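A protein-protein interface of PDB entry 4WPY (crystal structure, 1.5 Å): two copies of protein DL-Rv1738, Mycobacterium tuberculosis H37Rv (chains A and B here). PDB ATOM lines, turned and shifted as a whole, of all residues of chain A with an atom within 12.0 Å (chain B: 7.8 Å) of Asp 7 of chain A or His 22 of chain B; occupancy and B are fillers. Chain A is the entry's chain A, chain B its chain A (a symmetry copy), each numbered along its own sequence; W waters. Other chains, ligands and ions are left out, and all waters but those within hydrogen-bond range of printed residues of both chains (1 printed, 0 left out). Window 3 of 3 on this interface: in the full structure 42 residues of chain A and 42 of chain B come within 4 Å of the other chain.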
ATOM      1  N   ASP A   7      -1.810 -18.608 -19.650  1.00  0.00           N
ATOM      2  CA  ASP A   7      -2.882 -19.555 -19.357  1.00  0.00           C
ATOM      3  C   ASP A   7      -4.276 -18.895 -19.417  1.00  0.00           C
ATOM      4  O   ASP A   7      -5.295 -19.582 -19.524  1.00  0.00           O
ATOM      5  CB  ASP A   7      -2.646 -20.191 -17.982  1.00  0.00           C
ATOM      6  CG  ASP A   7      -3.021 -21.663 -17.952  1.00  0.00           C
ATOM      7  OD1 ASP A   7      -4.073 -22.019 -18.531  1.00  0.00           O
ATOM      8  OD2 ASP A   7      -2.254 -22.468 -17.366  1.00  0.00           O
ATOM      9  N   HIS A   8      -4.331 -17.570 -19.350  1.00  0.00           N
ATOM     10  CA  HIS A   8      -5.590 -16.852 -19.509  1.00  0.00           C
ATOM     11  C   HIS A   8      -5.713 -16.299 -20.919  1.00  0.00           C
ATOM     12  O   HIS A   8      -4.717 -15.968 -21.563  1.00  0.00           O
ATOM     13  CB  HIS A   8      -5.705 -15.702 -18.516  1.00  0.00           C
ATOM     14  CG  HIS A   8      -5.763 -16.138 -17.088  1.00  0.00           C
ATOM     15  ND1 HIS A   8      -6.848 -15.888 -16.274  1.00  0.00           N
ATOM     16  CD2 HIS A   8      -4.863 -16.808 -16.326  1.00  0.00           C
ATOM     17  CE1 HIS A   8      -6.612 -16.383 -15.069  1.00  0.00           C
ATOM     18  NE2 HIS A   8      -5.417 -16.951 -15.077  1.00  0.00           N
ATOM     19  N   VAL A   9      -6.951 -16.198 -21.393  1.00  0.00           N
ATOM     20  CA  VAL A   9      -7.263 -15.537 -22.655  1.00  0.00           C
ATOM     21  C   VAL A   9      -8.074 -14.306 -22.294  1.00  0.00           C
ATOM     22  O   VAL A   9      -9.145 -14.424 -21.691  1.00  0.00           O
ATOM     23  CB  VAL A   9      -8.040 -16.456 -23.607  1.00  0.00           C
ATOM     24  CG1 VAL A   9      -8.485 -15.679 -24.849  1.00  0.00           C
ATOM     25  CG2 VAL A   9      -7.190 -17.672 -23.987  1.00  0.00           C
ATOM     26  N   LEU A  10      -7.552 -13.131 -22.638  1.00  0.00           N
ATOM     27  CA  LEU A  10      -8.147 -11.852 -22.277  1.00  0.00           C
ATOM     28  C   LEU A  10      -8.738 -11.181 -23.509  1.00  0.00           C
ATOM     29  O   LEU A  10      -8.141 -11.207 -24.590  1.00  0.00           O
ATOM     30  CB  LEU A  10      -7.110 -10.924 -21.644  1.00  0.00           C
ATOM     31  CG  LEU A  10      -6.331 -11.568 -20.506  1.00  0.00           C
ATOM     32  CD1 LEU A  10      -5.387 -10.562 -19.911  1.00  0.00           C
ATOM     33  CD2 LEU A  10      -7.251 -12.097 -19.428  1.00  0.00           C
ATOM     34  N   GLN A  11      -9.913 -10.584 -23.341  1.00  0.00           N
ATOM     35  CA  GLN A  11     -10.524  -9.766 -24.377  1.00  0.00           C
ATOM     36  C   GLN A  11     -11.057  -8.492 -23.750  1.00  0.00           C
ATOM     37  O   GLN A  11     -11.309  -8.423 -22.545  1.00  0.00           O
ATOM     38  CB  GLN A  11     -11.685 -10.467 -25.072  1.00  0.00           C
ATOM     39  CG  GLN A  11     -11.301 -11.699 -25.805  1.00  0.00           C
ATOM     40  CD  GLN A  11     -12.509 -12.386 -26.325  1.00  0.00           C
ATOM     41  OE1 GLN A  11     -13.166 -11.896 -27.260  1.00  0.00           O
ATOM     42  NE2 GLN A  11     -12.857 -13.506 -25.701  1.00  0.00           N
ATOM     43  N   ILE B  19     -12.933  -9.392 -20.418  1.00  0.00           N
ATOM     44  CA  ILE B  19     -13.336 -10.786 -20.432  1.00  0.00           C
ATOM     45  C   ILE B  19     -12.087 -11.630 -20.223  1.00  0.00           C
ATOM     46  O   ILE B  19     -11.121 -11.508 -20.977  1.00  0.00           O
ATOM     47  CB  ILE B  19     -14.024 -11.171 -21.751  1.00  0.00           C
ATOM     48  CG1 ILE B  19     -15.179 -10.209 -22.087  1.00  0.00           C
ATOM     49  CG2 ILE B  19     -14.525 -12.607 -21.670  1.00  0.00           C
ATOM     50  CD1 ILE B  19     -15.735 -10.449 -23.457  1.00  0.00           C
ATOM     51  N   ASP B  20     -12.114 -12.494 -19.223  1.00  0.00           N
ATOM     52  CA  ASP B  20     -10.957 -13.300 -18.831  1.00  0.00           C
ATOM     53  C   ASP B  20     -11.394 -14.757 -18.827  1.00  0.00           C
ATOM     54  O   ASP B  20     -12.199 -15.144 -17.978  1.00  0.00           O
ATOM     55  CB  ASP B  20     -10.478 -12.833 -17.446  1.00  0.00           C
ATOM     56  CG  ASP B  20      -9.305 -13.624 -16.890  1.00  0.00           C
ATOM     57  OD1 ASP B  20      -8.991 -14.706 -17.360  1.00  0.00           O
ATOM     58  OD2 ASP B  20      -8.706 -13.157 -15.913  1.00  0.00           O
ATOM     59  N   GLU B  21     -10.881 -15.559 -19.784  1.00  0.00           N
ATOM     60  CA  GLU B  21     -11.151 -16.989 -19.878  1.00  0.00           C
ATOM     61  C   GLU B  21      -9.994 -17.754 -19.251  1.00  0.00           C
ATOM     62  O   GLU B  21      -8.832 -17.489 -19.567  1.00  0.00           O
ATOM     63  CB  GLU B  21     -11.291 -17.451 -21.334  1.00  0.00           C
ATOM     64  CG  GLU B  21     -12.300 -16.699 -22.205  1.00  0.00           C
ATOM     65  CD  GLU B  21     -12.165 -17.064 -23.687  1.00  0.00           C
ATOM     66  OE1 GLU B  21     -11.227 -17.813 -24.059  1.00  0.00           O
ATOM     67  OE2 GLU B  21     -12.996 -16.611 -24.488  1.00  0.00           O
ATOM     68  N   HIS B  22     -10.304 -18.703 -18.378  1.00  0.00           N
ATOM     69  CA  HIS B  22      -9.256 -19.514 -17.774  1.00  0.00           C
ATOM     70  C   HIS B  22      -9.853 -20.842 -17.364  1.00  0.00           C
ATOM     71  O   HIS B  22     -10.746 -20.882 -16.516  1.00  0.00           O
ATOM     72  CB  HIS B  22      -8.644 -18.794 -16.567  1.00  0.00           C
ATOM     73  CG  HIS B  22      -7.536 -19.553 -15.913  1.00  0.00           C
ATOM     74  ND1 HIS B  22      -6.397 -19.942 -16.586  1.00  0.00           N
ATOM     75  CD2 HIS B  22      -7.391 -19.991 -14.641  1.00  0.00           C
ATOM     76  CE1 HIS B  22      -5.600 -20.596 -15.758  1.00  0.00           C
ATOM     77  NE2 HIS B  22      -6.178 -20.637 -14.570  1.00  0.00           N
ATOM     78  N   GLU B  23      -9.377 -21.917 -17.991  1.00  0.00           N
ATOM     79  CA  GLU B  23      -9.703 -23.277 -17.573  1.00  0.00           C
ATOM     80  C   GLU B  23     -11.211 -23.498 -17.539  1.00  0.00           C
ATOM     81  O   GLU B  23     -11.736 -24.147 -16.636  1.00  0.00           O
ATOM     82  CB  GLU B  23      -9.074 -23.589 -16.216  1.00  0.00           C
ATOM     83  CG  GLU B  23      -7.556 -23.596 -16.278  1.00  0.00           C
ATOM     84  CD  GLU B  23      -6.902 -24.077 -15.004  1.00  0.00           C
ATOM     85  OE1 GLU B  23      -5.727 -24.481 -15.090  1.00  0.00           O
ATOM     86  OE2 GLU B  23      -7.542 -24.041 -13.930  1.00  0.00           O
ATOM     87  N   GLY B  24     -11.913 -22.941 -18.528  1.00  0.00           N
ATOM     88  CA  GLY B  24     -13.345 -23.118 -18.654  1.00  0.00           C
ATOM     89  C   GLY B  24     -14.195 -22.116 -17.895  1.00  0.00           C
ATOM     90  O   GLY B  24     -15.424 -22.107 -18.074  1.00  0.00           O
ATOM     91  N   LEU B  25     -13.593 -21.272 -17.067  1.00  0.00           N
ATOM     92  CA  LEU B  25     -14.310 -20.187 -16.387  1.00  0.00           C
ATOM     93  C   LEU B  25     -14.040 -18.872 -17.092  1.00  0.00           C
ATOM     94  O   LEU B  25     -12.884 -18.517 -17.318  1.00  0.00           O
ATOM     95  CB  LEU B  25     -13.879 -20.059 -14.919  1.00  0.00           C
ATOM     96  CG  LEU B  25     -14.540 -18.890 -14.180  1.00  0.00           C
ATOM     97  CD1 LEU B  25     -16.042 -19.137 -14.095  1.00  0.00           C
ATOM     98  CD2 LEU B  25     -13.918 -18.689 -12.828  1.00  0.00           C
ATOM     99  N   THR B  26     -15.097 -18.132 -17.406  1.00  0.00           N
ATOM    100  CA  THR B  26     -14.959 -16.829 -18.033  1.00  0.00           C
ATOM    101  C   THR B  26     -15.548 -15.784 -17.104  1.00  0.00           C
ATOM    102  O   THR B  26     -16.695 -15.900 -16.667  1.00  0.00           O
ATOM    103  CB  THR B  26     -15.631 -16.785 -19.418  1.00  0.00           C
ATOM    104  OG1 THR B  26     -15.051 -17.816 -20.213  1.00  0.00           O
ATOM    105  CG2 THR B  26     -15.353 -15.494 -20.099  1.00  0.00           C
ATOM    106  N   ARG B  27     -14.749 -14.786 -16.784  1.00  0.00           N
ATOM    107  CA  ARG B  27     -15.168 -13.685 -15.927  1.00  0.00           C
ATOM    108  C   ARG B  27     -15.188 -12.402 -16.736  1.00  0.00           C
ATOM    109  O   ARG B  27     -14.196 -12.067 -17.389  1.00  0.00           O
ATOM    110  CB  ARG B  27     -14.216 -13.530 -14.736  1.00  0.00           C
ATOM    111  CG  ARG B  27     -14.615 -12.394 -13.811  1.00  0.00           C
ATOM    112  CD  ARG B  27     -13.663 -12.267 -12.633  1.00  0.00           C
ATOM    113  NE  ARG B  27     -13.767 -13.396 -11.714  1.00  0.00           N
ATOM    114  CZ  ARG B  27     -13.001 -14.494 -11.743  1.00  0.00           C
ATOM    115  NH1 ARG B  27     -12.073 -14.661 -12.690  1.00  0.00           N
ATOM    116  NH2 ARG B  27     -13.183 -15.448 -10.827  1.00  0.00           N
ATOM    117  N   ALA B  45     -19.252 -17.056 -16.274  1.00  0.00           N
ATOM    118  CA  ALA B  45     -19.840 -18.164 -17.013  1.00  0.00           C
ATOM    119  C   ALA B  45     -18.819 -19.290 -17.042  1.00  0.00           C
ATOM    120  O   ALA B  45     -17.655 -19.076 -17.359  1.00  0.00           O
ATOM    121  CB  ALA B  45     -20.250 -17.770 -18.440  1.00  0.00           C
ATOM    122  N   ARG B  46     -19.254 -20.474 -16.711  1.00  0.00           N
ATOM    123  CA  ARG B  46     -18.389 -21.641 -16.762  1.00  0.00           C
ATOM    124  C   ARG B  46     -18.897 -22.587 -17.828  1.00  0.00           C
ATOM    125  O   ARG B  46     -20.087 -22.894 -17.865  1.00  0.00           O
ATOM    126  CB  ARG B  46     -18.326 -22.342 -15.414  1.00  0.00           C
ATOM    127  CG  ARG B  46     -17.231 -23.439 -15.437  1.00  0.00           C
ATOM    128  CD  ARG B  46     -17.007 -24.055 -14.140  1.00  0.00           C
ATOM    129  NE  ARG B  46     -16.439 -23.168 -13.140  1.00  0.00           N
ATOM    130  CZ  ARG B  46     -15.135 -23.031 -12.905  1.00  0.00           C
ATOM    131  NH1 ARG B  46     -14.242 -23.695 -13.634  1.00  0.00           N
ATOM    132  NH2 ARG B  46     -14.725 -22.205 -11.944  1.00  0.00           N
HETATM  133  O   HOH W   1     -11.327 -13.711 -23.076  1.00  0.00           O
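Water W1 lies within hydrogen-bond range of O of Val 9 of chain A, NE2 of Gln 11 of chain A and O of Ile 19 of chain B.
No position is printed for both chains.
The backbone NH (N) of Asp 20 of chain B is in hydrogen-bond range of the backbone carbonyl oxygen (O) of Arg 27 of chain B (2.8 Å).
His 8 of chain A touches Glu 21 of chain B (CA to O, 3.3 Å).
Val 9 of chain A touches Ile 19 of chain B.
Asp 20 of chain B touches Val 9 of chain A.
Leu 10 of chain A touches Ile 19 of chain B (CA to O, 3.3 Å).
Leu 10 of chain A touches Asp 20 of chain B (CD2 to CG, 3.6 Å).
N of Glu 21 of chain B lies within hydrogen-bond range of O of Val 9 of chain A (2.8 Å).
ND1 of His 22 of chain B is in hydrogen-bond range of O of Asp 7 of chain A.
The backbone carbonyl oxygen of Ile 19 of chain B lies within hydrogen-bond range of the backbone NH of Gln 11 of chain A (2.8 Å).
A ring nitrogen (NE2) of His 8 of chain A lies close to a ring nitrogen (ND1) of His 22 of chain B (3.5 Å).
The side-chain amide nitrogen of Gln 11 of chain A is in hydrogen-bond range of the side-chain carboxylate of Glu 21 of chain B, 3.3 Å away.
A ring nitrogen (ND1) of His 8 of chain A lies within hydrogen-bond range of the side-chain carboxylate (OD1) of Asp 20 of chain B, 2.7 Å away.
Hydrophobic or aromatic side chains of chain B that line the printed part of chain A: Ile 19 and His 22.
Asp 7 of chain A touches one residue of chain B.
Printed residues of chain B within 4 Å of His 8 of chain A: Asp 20 (2.7 Å), Glu 21 (3.3 Å) and His 22 (3.4 Å).
Printed residues of chain B within 4 Å of Val 9 of chain A: Ile 19, Asp 20 and Glu 21.
Printed residues of chain B within 4 Å of Leu 10 of chain A: Ile 19 (3.3 Å) and Asp 20 (3.6 Å).
Printed residues of chain B within 4 Å of Gln 11 of chain A: Ile 19 and Glu 21.
Of the printed residues of chain A, Ile 19 of chain B touches Val 9, Leu 10 and Gln 11.
No residue of chain A comes within 4 Å of Glu 23 of chain B.
No residue of chain A comes within 4 Å of Gly 24 of chain B.
Leu 25 of chain B touches none of the printed residues of chain A.
The nearest residue of chain A that does not touch His 22 of chain B is Val 9 of chain A (5.2 Å).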
